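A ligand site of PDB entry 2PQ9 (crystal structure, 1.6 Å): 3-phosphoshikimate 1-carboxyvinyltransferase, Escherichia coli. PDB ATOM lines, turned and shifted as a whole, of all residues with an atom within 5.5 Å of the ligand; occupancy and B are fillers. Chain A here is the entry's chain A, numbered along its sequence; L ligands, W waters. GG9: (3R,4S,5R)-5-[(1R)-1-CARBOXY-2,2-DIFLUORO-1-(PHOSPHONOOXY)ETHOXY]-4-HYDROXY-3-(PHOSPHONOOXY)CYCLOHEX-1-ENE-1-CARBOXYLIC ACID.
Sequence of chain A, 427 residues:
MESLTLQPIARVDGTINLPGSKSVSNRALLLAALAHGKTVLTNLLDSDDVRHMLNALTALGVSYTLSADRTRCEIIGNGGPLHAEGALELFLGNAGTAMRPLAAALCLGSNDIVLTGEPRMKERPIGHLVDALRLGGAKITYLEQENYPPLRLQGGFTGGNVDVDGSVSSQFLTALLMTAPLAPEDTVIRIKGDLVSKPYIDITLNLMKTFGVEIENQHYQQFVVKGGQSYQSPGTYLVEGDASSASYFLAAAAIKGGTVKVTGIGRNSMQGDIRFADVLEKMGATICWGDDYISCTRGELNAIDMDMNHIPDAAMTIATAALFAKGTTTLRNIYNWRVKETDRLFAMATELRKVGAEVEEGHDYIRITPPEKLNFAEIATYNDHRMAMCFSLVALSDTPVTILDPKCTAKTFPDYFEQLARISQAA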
ATOM      1  N   LYS A  22      -7.532 -24.619  29.841  1.00  0.00           N
ATOM      2  CA  LYS A  22      -7.514 -26.085  29.727  1.00  0.00           C
ATOM      3  C   LYS A  22      -6.234 -26.545  29.000  1.00  0.00           C
ATOM      4  O   LYS A  22      -5.622 -27.533  29.401  1.00  0.00           O
ATOM      5  CB  LYS A  22      -8.770 -26.570  28.984  1.00  0.00           C
ATOM      6  CG  LYS A  22      -8.758 -28.073  28.631  1.00  0.00           C
ATOM      7  CD  LYS A  22      -8.435 -28.322  27.155  1.00  0.00           C
ATOM      8  CE  LYS A  22      -9.644 -28.027  26.279  1.00  0.00           C
ATOM      9  NZ  LYS A  22      -9.317 -27.994  24.835  1.00  0.00           N
ATOM     10  N   SER A  23      -5.857 -25.822  27.944  1.00  0.00           N
ATOM     11  CA  SER A  23      -4.674 -26.193  27.158  1.00  0.00           C
ATOM     12  C   SER A  23      -3.423 -26.168  28.014  1.00  0.00           C
ATOM     13  O   SER A  23      -2.605 -27.081  27.962  1.00  0.00           O
ATOM     14  CB  SER A  23      -4.511 -25.252  25.952  1.00  0.00           C
ATOM     15  OG  SER A  23      -5.539 -25.467  24.988  1.00  0.00           O
ATOM     16  N   ARG A  27      -1.231 -29.666  29.871  1.00  0.00           N
ATOM     17  CA  ARG A  27       0.180 -29.784  29.514  1.00  0.00           C
ATOM     18  C   ARG A  27       1.009 -29.705  30.796  1.00  0.00           C
ATOM     19  O   ARG A  27       1.942 -30.488  30.982  1.00  0.00           O
ATOM     20  CB  ARG A  27       0.604 -28.640  28.573  1.00  0.00           C
ATOM     21  CG  ARG A  27       0.183 -28.863  27.108  1.00  0.00           C
ATOM     22  CD  ARG A  27       0.333 -27.528  26.399  1.00  0.00           C
ATOM     23  NE  ARG A  27       0.155 -27.547  24.935  1.00  0.00           N
ATOM     24  CZ  ARG A  27      -1.020 -27.602  24.315  1.00  0.00           C
ATOM     25  NH1 ARG A  27      -1.065 -27.575  22.984  1.00  0.00           N
ATOM     26  NH2 ARG A  27      -2.143 -27.727  25.015  1.00  0.00           N
ATOM     27  N   ASP A  49     -12.120 -32.241  31.423  1.00  0.00           N
ATOM     28  CA  ASP A  49     -10.857 -32.631  30.766  1.00  0.00           C
ATOM     29  C   ASP A  49      -9.699 -32.721  31.747  1.00  0.00           C
ATOM     30  O   ASP A  49      -8.859 -33.598  31.614  1.00  0.00           O
ATOM     31  CB  ASP A  49     -10.488 -31.642  29.664  1.00  0.00           C
ATOM     32  CG  ASP A  49     -11.285 -31.852  28.390  1.00  0.00           C
ATOM     33  OD1 ASP A  49     -12.151 -32.766  28.321  1.00  0.00           O
ATOM     34  OD2 ASP A  49     -11.012 -31.092  27.437  1.00  0.00           O
ATOM     35  N   ASN A  94     -13.473 -36.973  27.044  1.00  0.00           N
ATOM     36  CA  ASN A  94     -13.464 -36.289  25.757  1.00  0.00           C
ATOM     37  C   ASN A  94     -12.196 -35.434  25.613  1.00  0.00           C
ATOM     38  O   ASN A  94     -12.152 -34.571  24.740  1.00  0.00           O
ATOM     39  CB  ASN A  94     -14.667 -35.346  25.649  1.00  0.00           C
ATOM     40  CG  ASN A  94     -15.993 -36.078  25.671  1.00  0.00           C
ATOM     41  OD1 ASN A  94     -16.352 -36.783  24.725  1.00  0.00           O
ATOM     42  ND2 ASN A  94     -16.734 -35.918  26.745  1.00  0.00           N
ATOM     43  N   ALA A  95     -11.183 -35.693  26.442  1.00  0.00           N
ATOM     44  CA  ALA A  95      -9.989 -34.827  26.433  1.00  0.00           C
ATOM     45  C   ALA A  95      -8.895 -35.116  25.419  1.00  0.00           C
ATOM     46  O   ALA A  95      -8.116 -36.042  25.599  1.00  0.00           O
ATOM     47  CB  ALA A  95      -9.379 -34.796  27.831  1.00  0.00           C
ATOM     48  N   GLY A  96      -8.839 -34.295  24.365  1.00  0.00           N
ATOM     49  CA  GLY A  96      -7.798 -34.429  23.361  1.00  0.00           C
ATOM     50  C   GLY A  96      -6.430 -34.153  23.969  1.00  0.00           C
ATOM     51  O   GLY A  96      -5.436 -34.814  23.608  1.00  0.00           O
ATOM     52  N   THR A  97      -6.386 -33.230  24.928  1.00  0.00           N
ATOM     53  CA  THR A  97      -5.130 -32.885  25.570  1.00  0.00           C
ATOM     54  C   THR A  97      -4.639 -33.943  26.552  1.00  0.00           C
ATOM     55  O   THR A  97      -3.561 -33.798  27.128  1.00  0.00           O
ATOM     56  CB  THR A  97      -5.165 -31.488  26.265  1.00  0.00           C
ATOM     57  OG1 THR A  97      -6.202 -31.446  27.250  1.00  0.00           O
ATOM     58  CG2 THR A  97      -5.409 -30.392  25.235  1.00  0.00           C
ATOM     59  N   ARG A 100      -4.071 -37.388  23.151  1.00  0.00           N
ATOM     60  CA  ARG A 100      -2.938 -37.300  22.226  1.00  0.00           C
ATOM     61  C   ARG A 100      -1.604 -37.276  22.990  1.00  0.00           C
ATOM     62  O   ARG A 100      -0.731 -38.104  22.734  1.00  0.00           O
ATOM     63  CB  ARG A 100      -3.084 -36.092  21.278  1.00  0.00           C
ATOM     64  CG  ARG A 100      -4.028 -36.318  20.058  1.00  0.00           C
ATOM     65  CD  ARG A 100      -5.501 -36.585  20.460  1.00  0.00           C
ATOM     66  NE  ARG A 100      -6.404 -36.666  19.294  1.00  0.00           N
ATOM     67  CZ  ARG A 100      -6.970 -35.622  18.685  1.00  0.00           C
ATOM     68  NH1 ARG A 100      -7.766 -35.800  17.642  1.00  0.00           N
ATOM     69  NH2 ARG A 100      -6.762 -34.389  19.129  1.00  0.00           N
ATOM     70  N   MET A 121     -14.814 -39.664  21.439  1.00  0.00           N
ATOM     71  CA  MET A 121     -13.354 -39.722  21.330  1.00  0.00           C
ATOM     72  C   MET A 121     -12.923 -40.843  20.376  1.00  0.00           C
ATOM     73  O   MET A 121     -11.891 -40.731  19.698  1.00  0.00           O
ATOM     74  CB  MET A 121     -12.713 -39.907  22.714  1.00  0.00           C
ATOM     75  CG  MET A 121     -11.168 -40.019  22.708  1.00  0.00           C
ATOM     76  SD  MET A 121     -10.336 -38.614  21.939  1.00  0.00           S
ATOM     77  CE  MET A 121     -10.625 -37.279  23.133  1.00  0.00           C
ATOM     78  N   ARG A 124     -12.564 -39.378  16.951  1.00  0.00           N
ATOM     79  CA  ARG A 124     -11.615 -38.279  16.682  1.00  0.00           C
ATOM     80  C   ARG A 124     -10.317 -38.945  16.223  1.00  0.00           C
ATOM     81  O   ARG A 124      -9.775 -39.819  16.908  1.00  0.00           O
ATOM     82  CB  ARG A 124     -11.462 -37.405  17.931  1.00  0.00           C
ATOM     83  CG  ARG A 124     -12.794 -36.672  18.252  1.00  0.00           C
ATOM     84  CD  ARG A 124     -12.697 -35.650  19.377  1.00  0.00           C
ATOM     85  NE  ARG A 124     -11.721 -34.611  19.065  1.00  0.00           N
ATOM     86  CZ  ARG A 124     -11.207 -33.790  19.977  1.00  0.00           C
ATOM     87  NH1 ARG A 124     -10.305 -32.891  19.609  1.00  0.00           N
ATOM     88  NH2 ARG A 124     -11.615 -33.858  21.241  1.00  0.00           N
ATOM     89  N   VAL A 168      -4.214 -32.105   9.945  1.00  0.00           N
ATOM     90  CA  VAL A 168      -5.487 -32.338  10.630  1.00  0.00           C
ATOM     91  C   VAL A 168      -5.521 -31.807  12.067  1.00  0.00           C
ATOM     92  O   VAL A 168      -6.516 -31.218  12.499  1.00  0.00           O
ATOM     93  CB  VAL A 168      -5.800 -33.855  10.652  1.00  0.00           C
ATOM     94  CG1 VAL A 168      -7.010 -34.139  11.553  1.00  0.00           C
ATOM     95  CG2 VAL A 168      -6.078 -34.350   9.230  1.00  0.00           C
ATOM     96  N   SER A 169      -4.455 -32.026  12.817  1.00  0.00           N
ATOM     97  CA  SER A 169      -4.389 -31.541  14.188  1.00  0.00           C
ATOM     98  C   SER A 169      -2.974 -31.164  14.590  1.00  0.00           C
ATOM     99  O   SER A 169      -2.005 -31.809  14.183  1.00  0.00           O
ATOM    100  CB  SER A 169      -4.926 -32.601  15.184  1.00  0.00           C
ATOM    101  OG  SER A 169      -4.819 -32.144  16.524  1.00  0.00           O
ATOM    102  N   SER A 170      -2.844 -30.098  15.386  1.00  0.00           N
ATOM    103  CA  SER A 170      -1.554 -29.706  15.906  1.00  0.00           C
ATOM    104  C   SER A 170      -1.222 -30.592  17.109  1.00  0.00           C
ATOM    105  O   SER A 170      -0.064 -30.655  17.518  1.00  0.00           O
ATOM    106  CB  SER A 170      -1.545 -28.247  16.364  1.00  0.00           C
ATOM    107  OG  SER A 170      -2.388 -28.022  17.482  1.00  0.00           O
ATOM    108  N   GLN A 171      -2.211 -31.283  17.666  1.00  0.00           N
ATOM    109  CA  GLN A 171      -1.950 -32.085  18.849  1.00  0.00           C
ATOM    110  C   GLN A 171      -1.007 -33.258  18.651  1.00  0.00           C
ATOM    111  O   GLN A 171      -0.399 -33.712  19.616  1.00  0.00           O
ATOM    112  CB  GLN A 171      -3.260 -32.567  19.454  1.00  0.00           C
ATOM    113  CG  GLN A 171      -4.125 -31.415  19.951  1.00  0.00           C
ATOM    114  CD  GLN A 171      -5.238 -31.860  20.881  1.00  0.00           C
ATOM    115  OE1 GLN A 171      -5.407 -33.035  21.140  1.00  0.00           O
ATOM    116  NE2 GLN A 171      -5.991 -30.895  21.397  1.00  0.00           N
ATOM    117  N   THR A 174       2.321 -31.661  18.962  1.00  0.00           N
ATOM    118  CA  THR A 174       2.477 -31.340  20.369  1.00  0.00           C
ATOM    119  C   THR A 174       2.894 -32.563  21.197  1.00  0.00           C
ATOM    120  O   THR A 174       3.822 -32.494  22.003  1.00  0.00           O
ATOM    121  CB  THR A 174       1.169 -30.747  20.919  1.00  0.00           C
ATOM    122  OG1 THR A 174       1.173 -29.331  20.654  1.00  0.00           O
ATOM    123  CG2 THR A 174       1.018 -30.998  22.418  1.00  0.00           C
ATOM    124  N   VAL A 196      -1.695 -27.031  10.779  1.00  0.00           N
ATOM    125  CA  VAL A 196      -2.832 -26.232  11.216  1.00  0.00           C
ATOM    126  C   VAL A 196      -2.694 -25.910  12.707  1.00  0.00           C
ATOM    127  O   VAL A 196      -1.858 -26.514  13.411  1.00  0.00           O
ATOM    128  CB  VAL A 196      -4.186 -26.988  10.996  1.00  0.00           C
ATOM    129  CG1 VAL A 196      -4.403 -27.285   9.510  1.00  0.00           C
ATOM    130  CG2 VAL A 196      -4.200 -28.267  11.816  1.00  0.00           C
ATOM    131  N   SER A 197      -3.470 -24.931  13.163  1.00  0.00           N
ATOM    132  CA  SER A 197      -3.500 -24.552  14.572  1.00  0.00           C
ATOM    133  C   SER A 197      -2.118 -24.297  15.139  1.00  0.00           C
ATOM    134  O   SER A 197      -1.820 -24.669  16.286  1.00  0.00           O
ATOM    135  CB  SER A 197      -4.204 -25.651  15.373  1.00  0.00           C
ATOM    136  OG  SER A 197      -5.591 -25.732  15.002  1.00  0.00           O
ATOM    137  N   TYR A 200      -0.963 -23.350  18.888  1.00  0.00           N
ATOM    138  CA  TYR A 200      -0.950 -24.298  20.001  1.00  0.00           C
ATOM    139  C   TYR A 200       0.406 -24.939  20.179  1.00  0.00           C
ATOM    140  O   TYR A 200       0.754 -25.383  21.272  1.00  0.00           O
ATOM    141  CB  TYR A 200      -2.053 -25.378  19.851  1.00  0.00           C
ATOM    142  CG  TYR A 200      -3.443 -24.797  20.054  1.00  0.00           C
ATOM    143  CD1 TYR A 200      -4.188 -24.295  18.974  1.00  0.00           C
ATOM    144  CD2 TYR A 200      -4.020 -24.737  21.335  1.00  0.00           C
ATOM    145  CE1 TYR A 200      -5.477 -23.763  19.168  1.00  0.00           C
ATOM    146  CE2 TYR A 200      -5.310 -24.218  21.523  1.00  0.00           C
ATOM    147  CZ  TYR A 200      -6.034 -23.740  20.440  1.00  0.00           C
ATOM    148  OH  TYR A 200      -7.329 -23.270  20.618  1.00  0.00           O
ATOM    149  N   PRO A 312      -9.111 -21.578  15.625  1.00  0.00           N
ATOM    150  CA  PRO A 312     -10.273 -22.401  15.318  1.00  0.00           C
ATOM    151  C   PRO A 312     -11.406 -22.465  16.341  1.00  0.00           C
ATOM    152  O   PRO A 312     -12.589 -22.502  15.968  1.00  0.00           O
ATOM    153  CB  PRO A 312      -9.649 -23.766  15.007  1.00  0.00           C
ATOM    154  CG  PRO A 312      -8.473 -23.815  15.964  1.00  0.00           C
ATOM    155  CD  PRO A 312      -7.899 -22.398  15.836  1.00  0.00           C
ATOM    156  N   ASP A 313     -11.065 -22.483  17.629  1.00  0.00           N
ATOM    157  CA  ASP A 313     -12.113 -22.569  18.653  1.00  0.00           C
ATOM    158  C   ASP A 313     -12.807 -21.232  18.869  1.00  0.00           C
ATOM    159  O   ASP A 313     -14.052 -21.145  18.821  1.00  0.00           O
ATOM    160  CB  ASP A 313     -11.547 -23.079  19.975  1.00  0.00           C
ATOM    161  CG  ASP A 313     -11.279 -24.578  19.962  1.00  0.00           C
ATOM    162  OD1 ASP A 313     -10.567 -25.027  20.884  1.00  0.00           O
ATOM    163  OD2 ASP A 313     -11.788 -25.323  19.087  1.00  0.00           O
ATOM    164  N   ASN A 336     -10.736 -28.563  10.163  1.00  0.00           N
ATOM    165  CA  ASN A 336     -10.760 -29.432  11.331  1.00  0.00           C
ATOM    166  C   ASN A 336     -11.882 -29.225  12.357  1.00  0.00           C
ATOM    167  O   ASN A 336     -11.969 -29.944  13.364  1.00  0.00           O
ATOM    168  CB  ASN A 336      -9.352 -29.591  11.974  1.00  0.00           C
ATOM    169  CG  ASN A 336      -8.942 -28.451  12.856  1.00  0.00           C
ATOM    170  OD1 ASN A 336      -9.718 -27.538  13.168  1.00  0.00           O
ATOM    171  ND2 ASN A 336      -7.689 -28.513  13.314  1.00  0.00           N
ATOM    172  N   LYS A 340     -13.687 -32.490  15.629  1.00  0.00           N
ATOM    173  CA  LYS A 340     -13.546 -32.199  17.037  1.00  0.00           C
ATOM    174  C   LYS A 340     -14.694 -32.753  17.904  1.00  0.00           C
ATOM    175  O   LYS A 340     -15.063 -33.896  17.688  1.00  0.00           O
ATOM    176  CB  LYS A 340     -13.304 -30.709  17.197  1.00  0.00           C
ATOM    177  CG  LYS A 340     -11.875 -30.387  16.702  1.00  0.00           C
ATOM    178  CD  LYS A 340     -11.577 -28.926  16.584  1.00  0.00           C
ATOM    179  CE  LYS A 340     -10.083 -28.773  16.272  1.00  0.00           C
ATOM    180  NZ  LYS A 340      -9.653 -27.385  16.356  1.00  0.00           N
ATOM    181  N   GLU A 341     -15.241 -32.005  18.868  1.00  0.00           N
ATOM    182  CA  GLU A 341     -16.290 -32.575  19.723  1.00  0.00           C
ATOM    183  C   GLU A 341     -17.517 -33.025  18.950  1.00  0.00           C
ATOM    184  O   GLU A 341     -18.304 -33.830  19.454  1.00  0.00           O
ATOM    185  CB  GLU A 341     -16.683 -31.617  20.851  1.00  0.00           C
ATOM    186  CG  GLU A 341     -15.620 -31.571  21.954  1.00  0.00           C
ATOM    187  CD  GLU A 341     -15.396 -32.936  22.609  1.00  0.00           C
ATOM    188  OE1 GLU A 341     -16.103 -33.253  23.595  1.00  0.00           O
ATOM    189  OE2 GLU A 341     -14.514 -33.696  22.141  1.00  0.00           O
ATOM    190  N   ARG A 344     -18.303 -29.648  13.652  1.00  0.00           N
ATOM    191  CA  ARG A 344     -18.764 -28.298  13.955  1.00  0.00           C
ATOM    192  C   ARG A 344     -19.251 -27.484  12.761  1.00  0.00           C
ATOM    193  O   ARG A 344     -20.028 -26.547  12.921  1.00  0.00           O
ATOM    194  CB  ARG A 344     -17.697 -27.532  14.744  1.00  0.00           C
ATOM    195  CG  ARG A 344     -17.524 -28.086  16.161  1.00  0.00           C
ATOM    196  CD  ARG A 344     -16.227 -27.594  16.786  1.00  0.00           C
ATOM    197  NE  ARG A 344     -16.247 -27.873  18.227  1.00  0.00           N
ATOM    198  CZ  ARG A 344     -15.201 -27.681  19.024  1.00  0.00           C
ATOM    199  NH1 ARG A 344     -15.331 -27.946  20.335  1.00  0.00           N
ATOM    200  NH2 ARG A 344     -14.027 -27.223  18.539  1.00  0.00           N
ATOM    201  N   ASP A 384     -21.129 -30.990  22.686  1.00  0.00           N
ATOM    202  CA  ASP A 384     -20.011 -30.093  22.441  1.00  0.00           C
ATOM    203  C   ASP A 384     -20.129 -28.816  23.269  1.00  0.00           C
ATOM    204  O   ASP A 384     -20.986 -27.979  23.006  1.00  0.00           O
ATOM    205  CB  ASP A 384     -19.995 -29.732  20.942  1.00  0.00           C
ATOM    206  CG  ASP A 384     -18.803 -28.874  20.536  1.00  0.00           C
ATOM    207  OD1 ASP A 384     -18.025 -28.420  21.395  1.00  0.00           O
ATOM    208  OD2 ASP A 384     -18.672 -28.643  19.314  1.00  0.00           O
ATOM    209  N   HIS A 385     -19.246 -28.676  24.265  1.00  0.00           N
ATOM    210  CA  HIS A 385     -19.225 -27.489  25.134  1.00  0.00           C
ATOM    211  C   HIS A 385     -19.293 -26.168  24.367  1.00  0.00           C
ATOM    212  O   HIS A 385     -19.985 -25.239  24.798  1.00  0.00           O
ATOM    213  CB  HIS A 385     -17.954 -27.517  26.032  1.00  0.00           C
ATOM    214  CG  HIS A 385     -16.651 -27.540  25.287  1.00  0.00           C
ATOM    215  ND1 HIS A 385     -15.513 -26.946  25.784  1.00  0.00           N
ATOM    216  CD2 HIS A 385     -16.297 -28.090  24.097  1.00  0.00           C
ATOM    217  CE1 HIS A 385     -14.519 -27.120  24.937  1.00  0.00           C
ATOM    218  NE2 HIS A 385     -14.957 -27.812  23.905  1.00  0.00           N
ATOM    219  N   ARG A 386     -18.617 -26.063  23.220  1.00  0.00           N
ATOM    220  CA  ARG A 386     -18.637 -24.788  22.511  1.00  0.00           C
ATOM    221  C   ARG A 386     -19.956 -24.509  21.799  1.00  0.00           C
ATOM    222  O   ARG A 386     -20.286 -23.353  21.568  1.00  0.00           O
ATOM    223  CB  ARG A 386     -17.438 -24.688  21.569  1.00  0.00           C
ATOM    224  CG  ARG A 386     -16.126 -24.826  22.331  1.00  0.00           C
ATOM    225  CD  ARG A 386     -14.915 -24.232  21.587  1.00  0.00           C
ATOM    226  NE  ARG A 386     -13.735 -24.628  22.348  1.00  0.00           N
ATOM    227  CZ  ARG A 386     -13.320 -24.074  23.476  1.00  0.00           C
ATOM    228  NH1 ARG A 386     -12.249 -24.585  24.082  1.00  0.00           N
ATOM    229  NH2 ARG A 386     -13.929 -23.006  24.000  1.00  0.00           N
ATOM    230  N   LYS A 411     -16.874 -29.657  29.979  1.00  0.00           N
ATOM    231  CA  LYS A 411     -15.623 -30.115  29.384  1.00  0.00           C
ATOM    232  C   LYS A 411     -14.505 -29.115  29.735  1.00  0.00           C
ATOM    233  O   LYS A 411     -13.404 -29.540  30.087  1.00  0.00           O
ATOM    234  CB  LYS A 411     -15.763 -30.214  27.851  1.00  0.00           C
ATOM    235  CG  LYS A 411     -14.442 -30.603  27.134  1.00  0.00           C
ATOM    236  CD  LYS A 411     -14.612 -30.661  25.602  1.00  0.00           C
ATOM    237  CE  LYS A 411     -13.257 -30.588  24.846  1.00  0.00           C
ATOM    238  NZ  LYS A 411     -12.368 -31.758  25.064  1.00  0.00           N
ATOM    239  N   THR A 412     -14.816 -27.813  29.656  1.00  0.00           N
ATOM    240  CA  THR A 412     -13.846 -26.750  29.975  1.00  0.00           C
ATOM    241  C   THR A 412     -14.344 -25.637  30.889  1.00  0.00           C
ATOM    242  O   THR A 412     -13.551 -24.815  31.345  1.00  0.00           O
ATOM    243  CB  THR A 412     -13.365 -26.012  28.692  1.00  0.00           C
ATOM    244  OG1 THR A 412     -14.506 -25.444  28.025  1.00  0.00           O
ATOM    245  CG2 THR A 412     -12.626 -26.932  27.786  1.00  0.00           C
HETATM  246  C1  GG9 L   1      -5.708 -27.790  21.498  1.00  0.00           C
HETATM  247  C2  GG9 L   1      -5.538 -27.491  20.110  1.00  0.00           C
HETATM  248  C3  GG9 L   1      -6.767 -27.336  19.217  1.00  0.00           C
HETATM  249  C4  GG9 L   1      -8.085 -26.987  20.052  1.00  0.00           C
HETATM  250  C5  GG9 L   1      -8.299 -28.063  21.152  1.00  0.00           C
HETATM  251  C6  GG9 L   1      -7.062 -27.961  22.129  1.00  0.00           C
HETATM  252  C7  GG9 L   1      -4.480 -27.928  22.354  1.00  0.00           C
HETATM  253  O1  GG9 L   1      -6.917 -28.639  18.363  1.00  0.00           O
HETATM  254  O2  GG9 L   1      -9.174 -26.934  19.108  1.00  0.00           O
HETATM  255  O3  GG9 L   1      -9.509 -27.786  21.859  1.00  0.00           O
HETATM  256  O4  GG9 L   1      -3.482 -28.387  21.846  1.00  0.00           O
HETATM  257  O5  GG9 L   1      -4.572 -27.539  23.486  1.00  0.00           O
HETATM  258  P1  GG9 L   1      -6.280 -28.824  16.841  1.00  0.00           P
HETATM  259  O6  GG9 L   1      -4.759 -28.685  17.003  1.00  0.00           O
HETATM  260  O7  GG9 L   1      -6.935 -27.681  15.967  1.00  0.00           O
HETATM  261  O8  GG9 L   1      -6.726 -30.276  16.527  1.00  0.00           O
HETATM  262  C8  GG9 L   1     -10.719 -28.588  21.733  1.00  0.00           C
HETATM  263  C9  GG9 L   1     -11.125 -29.112  20.275  1.00  0.00           C
HETATM  264  C10 GG9 L   1     -11.863 -27.780  22.268  1.00  0.00           C
HETATM  265  O9  GG9 L   1     -11.611 -27.388  23.462  1.00  0.00           O
HETATM  266  O10 GG9 L   1     -12.903 -27.496  21.642  1.00  0.00           O
HETATM  267  P2  GG9 L   1      -9.590 -31.042  22.799  1.00  0.00           P
HETATM  268  O11 GG9 L   1     -10.413 -32.247  23.309  1.00  0.00           O
HETATM  269  O12 GG9 L   1      -8.593 -30.584  23.817  1.00  0.00           O
HETATM  270  O13 GG9 L   1      -8.926 -31.399  21.437  1.00  0.00           O
HETATM  271  O14 GG9 L   1     -10.618 -29.770  22.632  1.00  0.00           O
HETATM  272  F1  GG9 L   1     -10.158 -29.685  19.647  1.00  0.00           F
HETATM  273  F2  GG9 L   1     -12.199 -29.875  20.311  1.00  0.00           F
HETATM  274  O   HOH W   1      -7.889 -31.695  18.468  1.00  0.00           O
HETATM  275  O   HOH W   2      -1.458 -28.836  20.014  1.00  0.00           O
HETATM  276  O   HOH W   3      -8.272 -31.673  14.983  1.00  0.00           O
HETATM  277  O   HOH W   4      -8.627 -31.605  26.123  1.00  0.00           O
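An oxygen (O6) of the ligand sits at hydrogen-bond distance from the backbone NH (N) of Ser 170. The side-chain hydroxyl of Ser 170 lies within hydrogen-bond range of an oxygen (O6) of the ligand, 2.5 Å away. O7 of the ligand is in hydrogen-bond range of OG of Ser 197 (2.6 Å). The side-chain hydroxyl (OG) of Ser 169 is in hydrogen-bond range of an oxygen (O8) of the ligand (2.7 Å). The side-chain amino group (NZ) of Lys 411 lies within salt-bridge range of an oxygen (O11) of the ligand. NH1 of Arg 124 is in salt-bridge range of O13 of the ligand (2.7 Å). The side-chain hydroxyl of Ser 23 is in hydrogen-bond range of an oxygen (O5) of the ligand. O9 of the ligand lies within salt-bridge range of NZ of Lys 22 (2.7 Å). The side-chain amino group (NZ) of Lys 340 is in salt-bridge range of an oxygen (O7) of the ligand. An oxygen (O11) of the ligand lies within hydrogen-bond range of the backbone NH of Gly 96 (2.8 Å). An oxygen (O4) of the ligand lies within salt-bridge range of the guanidinium group (NH1) of Arg 27 (2.8 Å). The guanidinium group (NH1) of Arg 344 lies within salt-bridge range of an oxygen (O10) of the ligand, 2.8 Å away. The side-chain amide nitrogen (ND2) of Asn 336 lies within hydrogen-bond range of an oxygen (O7) of the ligand, 2.9 Å away. NH1 of Arg 386 lies within salt-bridge range of O9 of the ligand. OD1 of Asp 313 is in hydrogen-bond range of O2 of the ligand, at 3.0 Å. The side-chain amide nitrogen (NE2) of Gln 171 sits at hydrogen-bond distance from an oxygen (O13) of the ligand, 3.0 Å away. A ring nitrogen (NE2) of His 385 lies within hydrogen-bond range of an oxygen (O10) of the ligand (3.1 Å).
The side-chain amino group (NZ) of Lys 411 sits at hydrogen-bond distance from the backbone carbonyl oxygen (O) of Asn 94 (2.8 Å). The guanidinium group (NH2) of Arg 27 sits at hydrogen-bond distance from the backbone carbonyl oxygen (O) of Ser 23. OD1 of Asn 336 lies within hydrogen-bond range of NZ of Lys 340, at 3.2 Å. The guanidinium group (NH1) of Arg 27 is in hydrogen-bond range of the backbone carbonyl oxygen (O) of Tyr 200 (3.3 Å). The guanidinium group (NH2) of Arg 344 is in salt-bridge range of the side-chain carboxylate (OD2) of Asp 313 (3.0 Å). The side-chain carboxylate (OD2) of Asp 384 lies within salt-bridge range of the guanidinium group (NE) of Arg 344, 2.8 Å away. The backbone NH (N) of Arg 386 lies within hydrogen-bond range of the side-chain carboxylate (OD1) of Asp 384 (3.0 Å). The guanidinium group of Arg 100 is in hydrogen-bond range of the side-chain amide oxygen of Gln 171, at 2.8 Å.
An oxygen (O11) of the ligand sits close to the backbone carbonyl oxygen of Asn 94. Ala 95 touches the ligand (C to O11, 3.9 Å). Thr 97 touches the ligand (CG2 to O5, 3.4 Å). CD2 of Tyr 200 touches C2 of the ligand, at 3.4 Å. Glu 341 touches the ligand (N to F2, 3.98 Å). Hydrophobic or aromatic side chains that line the ligand: Tyr 200 and His 385. The nearest printed residue that does not touch the ligand is Val 168 (4.1 Å).
Water W4 lies within hydrogen-bond range of an oxygen (O12) of the ligand (2.5 Å), the side-chain hydroxyl (OG1) of Thr 97 (2.7 Å), the side-chain carboxylate (OD2) of Asp 49 (2.8 Å) and the backbone NH (N) of Gly 96 (3.2 Å). Water W3 bridges an oxygen (O8) of the ligand (2.6 Å) and the backbone carbonyl oxygen of Val 168 (3.1 Å). Water W1 lies within hydrogen-bond range of O8 of the ligand (2.7 Å), NH1 of Arg 124 (2.9 Å) and NH2 of Arg 100 (3.0 Å). Water W2 lies within hydrogen-bond range of the side-chain hydroxyl (OG1) of Thr 174 (2.8 Å), an oxygen (O4) of the ligand (2.8 Å), the side-chain hydroxyl (OG) of Ser 170 (2.8 Å), the guanidinium group (NH1) of Arg 27 (3.3 Å) and the backbone NH (N) of Gln 171 (3.5 Å).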
